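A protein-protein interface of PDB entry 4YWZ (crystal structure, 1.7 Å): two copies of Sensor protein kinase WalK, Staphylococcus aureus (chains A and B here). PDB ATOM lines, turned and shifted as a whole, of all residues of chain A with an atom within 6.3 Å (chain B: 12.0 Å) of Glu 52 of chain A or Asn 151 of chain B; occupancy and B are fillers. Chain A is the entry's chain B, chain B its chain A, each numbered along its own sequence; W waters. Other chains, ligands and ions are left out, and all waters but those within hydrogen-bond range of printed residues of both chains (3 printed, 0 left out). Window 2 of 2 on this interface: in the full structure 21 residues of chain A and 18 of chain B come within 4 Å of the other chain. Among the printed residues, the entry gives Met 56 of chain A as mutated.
The side-chain amide nitrogen (NE2) of Gln 146 of chain B lies within hydrogen-bond range of the backbone carbonyl oxygen (O) of Glu 52 of chain A (3.2 Å). NE2 of Gln 146 of chain B lies within hydrogen-bond range of O of Tyr 53 of chain A, at 3.5 Å. O of Glu 52 of chain A lies within hydrogen-bond range of ND2 of Asn 149 of chain B. The side-chain amide nitrogen of Asn 55 of chain A sits close to the side-chain amide nitrogen of Asn 149 of chain B.
ND2 of Asn 48 of chain A lies within hydrogen-bond range of OE2 of Glu 52 of chain A (3.0 Å). The backbone carbonyl oxygen (O) of Ser 51 of chain A sits at hydrogen-bond distance from the side-chain amide nitrogen (ND2) of Asn 55 of chain A (3.3 Å).
Ile 150 of chain B touches Glu 52 of chain A. Glu 52 of chain A touches Asn 151 of chain B (OE2 to ND2, 3.6 Å). Ile 150 of chain B touches Tyr 53 of chain A. Asn 55 of chain A touches Gln 146 of chain B. CB of Met 56 of chain A touches NE2 of Gln 146 of chain B (3.6 Å).
No residue of chain B comes within 4 Å of Asn 48 of chain A. No residue of chain B comes within 4 Å of Leu 49 of chain A. No residue of chain B comes within 4 Å of Ser 51 of chain A. Tyr 53 of chain A touches two residues of chain B. No residue of chain B comes within 4 Å of Ala 54 of chain A. Printed residues of chain B within 4 Å of Met 56 of chain A: Gln 146 (3.6 Å). Of the printed residues of chain A, Gln 146 of chain B touches Glu 52, Tyr 53, Asn 55 and Met 56. Printed residues of chain A within 4 Å of Asn 149 of chain B: Glu 52 (2.9 Å) and Asn 55 (3.1 Å). Printed residues of chain A within 4 Å of Ile 150 of chain B: Glu 52 (3.8 Å) and Tyr 53 (3.8 Å). Asn 151 of chain B touches just one residue of chain A: Glu 52.
Printed residues of chain B that touch a printed residue of chain A: Gln 146, Asn 149, Ile 150 and Asn 151. Hydrophobic or aromatic side chains of chain B that line the printed part of chain A: Ile 150. Among the printed residues, no Asp or Glu carboxylate lies within 4 Å of a Lys or Arg side-chain nitrogen of the other chain.
No position is printed for both chains. Of the 9 pairs that touch across the chains among the printed residues, none has its exchanged pair printed and touching as well.
Water W1 lies within hydrogen-bond range of OE1 of Glu 52 of chain A (2.6 Å) and ND2 of Asn 151 of chain B (3.0 Å). Water W3 lies within hydrogen-bond range of OH of Tyr 53 of chain A (2.6 Å), O of Ile 150 of chain B (2.9 Å) and OE1 of Gln 152 of chain B (3.0 Å). Water W2 lies within hydrogen-bond range of the backbone carbonyl oxygen (O) of Asn 149 of chain B (2.7 Å) and the side-chain carboxylate (OE2) of Glu 52 of chain A (3.2 Å).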
ATOM      1  N   GLN A  47      26.203  -6.273  23.989  1.00  0.00           N
ATOM      2  CA  GLN A  47      25.899  -5.484  25.233  1.00  0.00           C
ATOM      3  C   GLN A  47      24.440  -5.184  25.385  1.00  0.00           C
ATOM      4  O   GLN A  47      23.893  -5.342  26.461  1.00  0.00           O
ATOM      5  CB  GLN A  47      26.673  -4.192  25.292  1.00  0.00           C
ATOM      6  CG  GLN A  47      26.476  -3.393  26.585  1.00  0.00           C
ATOM      7  CD  GLN A  47      27.088  -4.080  27.804  1.00  0.00           C
ATOM      8  OE1 GLN A  47      28.286  -4.344  27.857  1.00  0.00           O
ATOM      9  NE2 GLN A  47      26.245  -4.444  28.755  1.00  0.00           N
ATOM     10  N   ASN A  48      23.751  -4.794  24.298  1.00  0.00           N
ATOM     11  CA  ASN A  48      22.372  -4.529  24.453  1.00  0.00           C
ATOM     12  C   ASN A  48      21.649  -5.804  24.784  1.00  0.00           C
ATOM     13  O   ASN A  48      20.707  -5.790  25.609  1.00  0.00           O
ATOM     14  CB  ASN A  48      21.794  -3.824  23.234  1.00  0.00           C
ATOM     15  CG  ASN A  48      20.297  -3.618  23.355  1.00  0.00           C
ATOM     16  OD1 ASN A  48      19.808  -2.808  24.146  1.00  0.00           O
ATOM     17  ND2 ASN A  48      19.565  -4.403  22.609  1.00  0.00           N
ATOM     18  N   LEU A  49      22.055  -6.950  24.199  1.00  0.00           N
ATOM     19  CA  LEU A  49      21.292  -8.128  24.510  1.00  0.00           C
ATOM     20  C   LEU A  49      21.477  -8.464  26.013  1.00  0.00           C
ATOM     21  O   LEU A  49      20.509  -8.875  26.730  1.00  0.00           O
ATOM     22  CB  LEU A  49      21.700  -9.290  23.604  1.00  0.00           C
ATOM     23  CG  LEU A  49      21.045  -9.293  22.195  1.00  0.00           C
ATOM     24  CD1 LEU A  49      21.931 -10.264  21.362  1.00  0.00           C
ATOM     25  CD2 LEU A  49      19.641  -9.823  22.235  1.00  0.00           C
ATOM     26  N   LEU A  50      22.707  -8.390  26.453  1.00  0.00           N
ATOM     27  CA  LEU A  50      23.004  -8.812  27.864  1.00  0.00           C
ATOM     28  C   LEU A  50      22.175  -7.955  28.808  1.00  0.00           C
ATOM     29  O   LEU A  50      21.507  -8.457  29.741  1.00  0.00           O
ATOM     30  CB  LEU A  50      24.482  -8.663  28.235  1.00  0.00           C
ATOM     31  CG  LEU A  50      25.554  -9.501  27.551  1.00  0.00           C
ATOM     32  CD1 LEU A  50      26.873  -9.330  28.285  1.00  0.00           C
ATOM     33  CD2 LEU A  50      25.271 -10.971  27.412  1.00  0.00           C
ATOM     34  N   SER A  51      22.212  -6.665  28.537  1.00  0.00           N
ATOM     35  CA  SER A  51      21.432  -5.709  29.349  1.00  0.00           C
ATOM     36  C   SER A  51      19.911  -5.951  29.420  1.00  0.00           C
ATOM     37  O   SER A  51      19.342  -5.919  30.530  1.00  0.00           O
ATOM     38  CB  SER A  51      21.791  -4.326  28.869  1.00  0.00           C
ATOM     39  OG  SER A  51      23.139  -4.138  29.294  1.00  0.00           O
ATOM     40  N   GLU A  52      19.288  -6.312  28.292  1.00  0.00           N
ATOM     41  CA  GLU A  52      17.873  -6.574  28.246  1.00  0.00           C
ATOM     42  C   GLU A  52      17.574  -7.749  29.097  1.00  0.00           C
ATOM     43  O   GLU A  52      16.574  -7.796  29.818  1.00  0.00           O
ATOM     44  CB  GLU A  52      17.461  -6.898  26.818  1.00  0.00           C
ATOM     45  CG  GLU A  52      17.579  -5.703  25.866  1.00  0.00           C
ATOM     46  CD  GLU A  52      17.209  -6.031  24.416  1.00  0.00           C
ATOM     47  OE1 GLU A  52      17.190  -7.217  23.998  1.00  0.00           O
ATOM     48  OE2 GLU A  52      16.884  -5.093  23.654  1.00  0.00           O
ATOM     49  N   TYR A  53      18.406  -8.790  28.927  1.00  0.00           N
ATOM     50  CA  TYR A  53      18.207 -10.015  29.685  1.00  0.00           C
ATOM     51  C   TYR A  53      18.390  -9.877  31.232  1.00  0.00           C
ATOM     52  O   TYR A  53      17.611 -10.553  32.040  1.00  0.00           O
ATOM     53  CB  TYR A  53      19.019 -11.189  29.067  1.00  0.00           C
ATOM     54  CG  TYR A  53      18.360 -11.800  27.881  1.00  0.00           C
ATOM     55  CD1 TYR A  53      17.659 -12.995  27.969  1.00  0.00           C
ATOM     56  CD2 TYR A  53      18.491 -11.236  26.630  1.00  0.00           C
ATOM     57  CE1 TYR A  53      17.071 -13.567  26.864  1.00  0.00           C
ATOM     58  CE2 TYR A  53      17.847 -11.782  25.531  1.00  0.00           C
ATOM     59  CZ  TYR A  53      17.199 -12.980  25.650  1.00  0.00           C
ATOM     60  OH  TYR A  53      16.630 -13.555  24.540  1.00  0.00           O
ATOM     61  N   ALA A  54      19.299  -8.990  31.625  1.00  0.00           N
ATOM     62  CA  ALA A  54      19.639  -8.818  33.021  1.00  0.00           C
ATOM     63  C   ALA A  54      18.586  -7.985  33.767  1.00  0.00           C
ATOM     64  O   ALA A  54      18.587  -7.982  34.984  1.00  0.00           O
ATOM     65  CB  ALA A  54      21.014  -8.225  33.226  1.00  0.00           C
ATOM     66  N   ASN A  55      17.668  -7.369  33.017  1.00  0.00           N
ATOM     67  CA  ASN A  55      16.590  -6.625  33.655  1.00  0.00           C
ATOM     68  C   ASN A  55      15.605  -7.496  34.350  1.00  0.00           C
ATOM     69  O   ASN A  55      14.796  -6.984  35.114  1.00  0.00           O
ATOM     70  CB  ASN A  55      15.819  -5.797  32.602  1.00  0.00           C
ATOM     71  CG  ASN A  55      16.553  -4.495  32.262  1.00  0.00           C
ATOM     72  OD1 ASN A  55      17.040  -3.782  33.166  1.00  0.00           O
ATOM     73  ND2 ASN A  55      16.625  -4.170  30.964  1.00  0.00           N
ATOM     74  N   MET A  56      15.587  -8.790  34.042  1.00  0.00           N
ATOM     75  CA  MET A  56      14.725  -9.673  34.794  1.00  0.00           C
ATOM     76  C   MET A  56      15.148  -9.685  36.251  1.00  0.00           C
ATOM     77  O   MET A  56      16.342  -9.634  36.598  1.00  0.00           O
ATOM     78  CB  MET A  56      14.579 -11.043  34.173  1.00  0.00           C
ATOM     79  CG  MET A  56      15.804 -11.880  33.885  1.00  0.00           C
ATOM     80  SD  MET A  56      15.157 -13.753  33.891  1.00  0.00           S
ATOM     81  CE  MET A  56      14.217 -13.701  35.595  1.00  0.00           C
ATOM     82  N   THR A  75      26.808  -6.763  32.501  1.00  0.00           N
ATOM     83  CA  THR A  75      25.654  -5.977  32.736  1.00  0.00           C
ATOM     84  C   THR A  75      25.764  -5.111  33.980  1.00  0.00           C
ATOM     85  O   THR A  75      24.872  -4.250  34.185  1.00  0.00           O
ATOM     86  CB  THR A  75      24.433  -6.841  32.910  1.00  0.00           C
ATOM     87  OG1 THR A  75      24.617  -7.788  33.990  1.00  0.00           O
ATOM     88  CG2 THR A  75      24.161  -7.590  31.662  1.00  0.00           C
ATOM     89  N   ASN B   6       9.106 -20.712  21.283  1.00  0.00           N
ATOM     90  CA  ASN B   6       8.110 -21.160  22.337  1.00  0.00           C
ATOM     91  C   ASN B   6       8.377 -20.612  23.730  1.00  0.00           C
ATOM     92  O   ASN B   6       7.801 -21.124  24.729  1.00  0.00           O
ATOM     93  CB  ASN B   6       8.115 -22.678  22.443  1.00  0.00           C
ATOM     94  CG  ASN B   6       7.014 -23.294  21.624  1.00  0.00           C
ATOM     95  OD1 ASN B   6       5.894 -23.473  22.112  1.00  0.00           O
ATOM     96  ND2 ASN B   6       7.302 -23.575  20.364  1.00  0.00           N
ATOM     97  N   LEU B   7       9.233 -19.622  23.780  1.00  0.00           N
ATOM     98  CA  LEU B   7       9.783 -19.114  25.003  1.00  0.00           C
ATOM     99  C   LEU B   7       8.627 -18.502  25.835  1.00  0.00           C
ATOM    100  O   LEU B   7       8.543 -18.699  27.078  1.00  0.00           O
ATOM    101  CB  LEU B   7      10.812 -18.063  24.717  1.00  0.00           C
ATOM    102  CG  LEU B   7      11.421 -17.391  25.932  1.00  0.00           C
ATOM    103  CD1 LEU B   7      12.150 -18.368  26.861  1.00  0.00           C
ATOM    104  CD2 LEU B   7      12.323 -16.235  25.576  1.00  0.00           C
ATOM    105  N   GLU B   8       7.713 -17.821  25.144  1.00  0.00           N
ATOM    106  CA  GLU B   8       6.575 -17.184  25.850  1.00  0.00           C
ATOM    107  C   GLU B   8       5.723 -18.215  26.572  1.00  0.00           C
ATOM    108  O   GLU B   8       5.411 -18.053  27.790  1.00  0.00           O
ATOM    109  CB  GLU B   8       5.742 -16.283  24.893  1.00  0.00           C
ATOM    110  CG  GLU B   8       4.528 -15.726  25.634  1.00  0.00           C
ATOM    111  CD  GLU B   8       3.729 -14.751  24.786  1.00  0.00           C
ATOM    112  OE1 GLU B   8       4.325 -14.198  23.847  1.00  0.00           O
ATOM    113  OE2 GLU B   8       2.543 -14.558  25.091  1.00  0.00           O
ATOM    114  N   LYS B   9       5.382 -19.325  25.936  1.00  0.00           N
ATOM    115  CA  LYS B   9       4.516 -20.316  26.560  1.00  0.00           C
ATOM    116  C   LYS B   9       5.232 -20.998  27.698  1.00  0.00           C
ATOM    117  O   LYS B   9       4.663 -21.271  28.767  1.00  0.00           O
ATOM    118  CB  LYS B   9       4.064 -21.335  25.493  1.00  0.00           C
ATOM    119  CG  LYS B   9       3.314 -22.520  26.065  1.00  0.00           C
ATOM    120  CD  LYS B   9       3.253 -23.665  25.053  1.00  0.00           C
ATOM    121  CE  LYS B   9       2.890 -24.980  25.727  1.00  0.00           C
ATOM    122  NZ  LYS B   9       1.647 -24.754  26.510  1.00  0.00           N
ATOM    123  N   LEU B  11       7.666 -19.701  29.668  1.00  0.00           N
ATOM    124  CA  LEU B  11       7.820 -18.791  30.791  1.00  0.00           C
ATOM    125  C   LEU B  11       6.472 -18.611  31.471  1.00  0.00           C
ATOM    126  O   LEU B  11       6.449 -18.550  32.706  1.00  0.00           O
ATOM    127  CB  LEU B  11       8.407 -17.492  30.379  1.00  0.00           C
ATOM    128  CG  LEU B  11       9.846 -17.590  29.838  1.00  0.00           C
ATOM    129  CD1 LEU B  11      10.225 -16.189  29.460  1.00  0.00           C
ATOM    130  CD2 LEU B  11      10.748 -18.141  30.919  1.00  0.00           C
ATOM    131  N   ASP B 142       4.653  -9.343  34.970  1.00  0.00           N
ATOM    132  CA  ASP B 142       6.087  -9.300  34.993  1.00  0.00           C
ATOM    133  C   ASP B 142       6.715 -10.183  33.913  1.00  0.00           C
ATOM    134  O   ASP B 142       7.795  -9.804  33.405  1.00  0.00           O
ATOM    135  CB  ASP B 142       6.628  -9.663  36.394  1.00  0.00           C
ATOM    136  CG  ASP B 142       6.411  -8.555  37.523  1.00  0.00           C
ATOM    137  OD1 ASP B 142       6.284  -7.319  37.248  1.00  0.00           O
ATOM    138  OD2 ASP B 142       6.565  -9.014  38.696  1.00  0.00           O
ATOM    139  N   VAL B 143       6.099 -11.342  33.530  1.00  0.00           N
ATOM    140  CA  VAL B 143       6.510 -12.216  32.436  1.00  0.00           C
ATOM    141  C   VAL B 143       6.363 -11.475  31.092  1.00  0.00           C
ATOM    142  O   VAL B 143       7.298 -11.362  30.326  1.00  0.00           O
ATOM    143  CB  VAL B 143       5.767 -13.554  32.408  1.00  0.00           C
ATOM    144  CG1 VAL B 143       6.312 -14.333  31.276  1.00  0.00           C
ATOM    145  CG2 VAL B 143       5.940 -14.234  33.822  1.00  0.00           C
ATOM    146  N   TYR B 144       5.164 -10.941  30.837  1.00  0.00           N
ATOM    147  CA  TYR B 144       4.938 -10.188  29.601  1.00  0.00           C
ATOM    148  C   TYR B 144       5.851  -9.019  29.445  1.00  0.00           C
ATOM    149  O   TYR B 144       6.395  -8.781  28.340  1.00  0.00           O
ATOM    150  CB  TYR B 144       3.448  -9.809  29.542  1.00  0.00           C
ATOM    151  CG  TYR B 144       2.470 -10.968  29.374  1.00  0.00           C
ATOM    152  CD1 TYR B 144       2.322 -11.662  28.156  1.00  0.00           C
ATOM    153  CD2 TYR B 144       1.673 -11.333  30.384  1.00  0.00           C
ATOM    154  CE1 TYR B 144       1.370 -12.682  28.061  1.00  0.00           C
ATOM    155  CE2 TYR B 144       0.714 -12.358  30.262  1.00  0.00           C
ATOM    156  CZ  TYR B 144       0.575 -12.992  29.118  1.00  0.00           C
ATOM    157  OH  TYR B 144      -0.348 -13.996  29.060  1.00  0.00           O
ATOM    158  N   ASN B 145       6.105  -8.312  30.528  1.00  0.00           N
ATOM    159  CA  ASN B 145       7.007  -7.143  30.524  1.00  0.00           C
ATOM    160  C   ASN B 145       8.430  -7.568  30.157  1.00  0.00           C
ATOM    161  O   ASN B 145       9.107  -6.947  29.364  1.00  0.00           O
ATOM    162  CB  ASN B 145       7.039  -6.377  31.812  1.00  0.00           C
ATOM    163  CG  ASN B 145       5.783  -5.498  32.066  1.00  0.00           C
ATOM    164  OD1 ASN B 145       5.100  -5.100  31.130  1.00  0.00           O
ATOM    165  ND2 ASN B 145       5.487  -5.293  33.309  1.00  0.00           N
ATOM    166  N   GLN B 146       8.869  -8.673  30.747  1.00  0.00           N
ATOM    167  CA  GLN B 146      10.249  -9.139  30.443  1.00  0.00           C
ATOM    168  C   GLN B 146      10.341  -9.624  28.995  1.00  0.00           C
ATOM    169  O   GLN B 146      11.353  -9.380  28.347  1.00  0.00           O
ATOM    170  CB  GLN B 146      10.662 -10.134  31.479  1.00  0.00           C
ATOM    171  CG  GLN B 146      12.098 -10.607  31.192  1.00  0.00           C
ATOM    172  CD  GLN B 146      13.207  -9.539  31.181  1.00  0.00           C
ATOM    173  OE1 GLN B 146      13.013  -8.358  31.548  1.00  0.00           O
ATOM    174  NE2 GLN B 146      14.430 -10.006  30.739  1.00  0.00           N
ATOM    175  N   LEU B 147       9.335 -10.302  28.486  1.00  0.00           N
ATOM    176  CA  LEU B 147       9.336 -10.789  27.099  1.00  0.00           C
ATOM    177  C   LEU B 147       9.423  -9.588  26.162  1.00  0.00           C
ATOM    178  O   LEU B 147      10.136  -9.577  25.154  1.00  0.00           O
ATOM    179  CB  LEU B 147       8.100 -11.627  26.840  1.00  0.00           C
ATOM    180  CG  LEU B 147       8.068 -13.024  27.427  1.00  0.00           C
ATOM    181  CD1 LEU B 147       6.713 -13.652  27.309  1.00  0.00           C
ATOM    182  CD2 LEU B 147       9.038 -13.828  26.578  1.00  0.00           C
ATOM    183  N   ASN B 148       8.680  -8.526  26.485  1.00  0.00           N
ATOM    184  CA  ASN B 148       8.711  -7.341  25.608  1.00  0.00           C
ATOM    185  C   ASN B 148      10.046  -6.691  25.679  1.00  0.00           C
ATOM    186  O   ASN B 148      10.597  -6.237  24.659  1.00  0.00           O
ATOM    187  CB  ASN B 148       7.622  -6.330  26.028  1.00  0.00           C
ATOM    188  CG  ASN B 148       6.256  -6.661  25.446  1.00  0.00           C
ATOM    189  OD1 ASN B 148       6.103  -7.274  24.383  1.00  0.00           O
ATOM    190  ND2 ASN B 148       5.231  -6.301  26.199  1.00  0.00           N
ATOM    191  N   ASN B 149      10.691  -6.685  26.846  1.00  0.00           N
ATOM    192  CA  ASN B 149      12.001  -6.104  26.964  1.00  0.00           C
ATOM    193  C   ASN B 149      13.118  -6.831  26.140  1.00  0.00           C
ATOM    194  O   ASN B 149      14.096  -6.235  25.785  1.00  0.00           O
ATOM    195  CB  ASN B 149      12.418  -6.183  28.410  1.00  0.00           C
ATOM    196  CG  ASN B 149      13.546  -5.333  28.738  1.00  0.00           C
ATOM    197  OD1 ASN B 149      13.638  -4.191  28.282  1.00  0.00           O
ATOM    198  ND2 ASN B 149      14.419  -5.832  29.571  1.00  0.00           N
ATOM    199  N   ILE B 150      12.966  -8.121  25.908  1.00  0.00           N
ATOM    200  CA  ILE B 150      13.938  -8.893  25.118  1.00  0.00           C
ATOM    201  C   ILE B 150      13.450  -9.130  23.708  1.00  0.00           C
ATOM    202  O   ILE B 150      13.977  -9.995  22.986  1.00  0.00           O
ATOM    203  CB  ILE B 150      14.305 -10.269  25.789  1.00  0.00           C
ATOM    204  CG1 ILE B 150      13.128 -11.202  25.853  1.00  0.00           C
ATOM    205  CG2 ILE B 150      14.898 -10.034  27.144  1.00  0.00           C
ATOM    206  CD1 ILE B 150      13.440 -12.626  26.318  1.00  0.00           C
ATOM    207  N   ASN B 151      12.357  -8.451  23.322  1.00  0.00           N
ATOM    208  CA  ASN B 151      11.736  -8.653  21.997  1.00  0.00           C
ATOM    209  C   ASN B 151      11.366 -10.065  21.620  1.00  0.00           C
ATOM    210  O   ASN B 151      11.677 -10.539  20.533  1.00  0.00           O
ATOM    211  CB  ASN B 151      12.596  -7.928  20.941  1.00  0.00           C
ATOM    212  CG  ASN B 151      12.794  -6.471  21.299  1.00  0.00           C
ATOM    213  OD1 ASN B 151      11.843  -5.686  21.288  1.00  0.00           O
ATOM    214  ND2 ASN B 151      13.997  -6.105  21.680  1.00  0.00           N
ATOM    215  N   GLN B 152      10.685 -10.761  22.543  1.00  0.00           N
ATOM    216  CA  GLN B 152      10.142 -12.047  22.314  1.00  0.00           C
ATOM    217  C   GLN B 152       8.662 -11.885  22.738  1.00  0.00           C
ATOM    218  O   GLN B 152       8.028 -12.907  22.846  1.00  0.00           O
ATOM    219  CB  GLN B 152      10.895 -13.148  23.140  1.00  0.00           C
ATOM    220  CG  GLN B 152      12.429 -13.163  22.967  1.00  0.00           C
ATOM    221  CD  GLN B 152      12.899 -13.809  21.661  1.00  0.00           C
ATOM    222  OE1 GLN B 152      14.011 -13.549  21.185  1.00  0.00           O
ATOM    223  NE2 GLN B 152      12.066 -14.697  21.101  1.00  0.00           N
HETATM  224  O   HOH W   1      16.441  -7.916  21.612  1.00  0.00           O
HETATM  225  O   HOH W   2      14.577  -3.643  25.370  1.00  0.00           O
HETATM  226  O   HOH W   3      16.067 -11.899  22.558  1.00  0.00           O
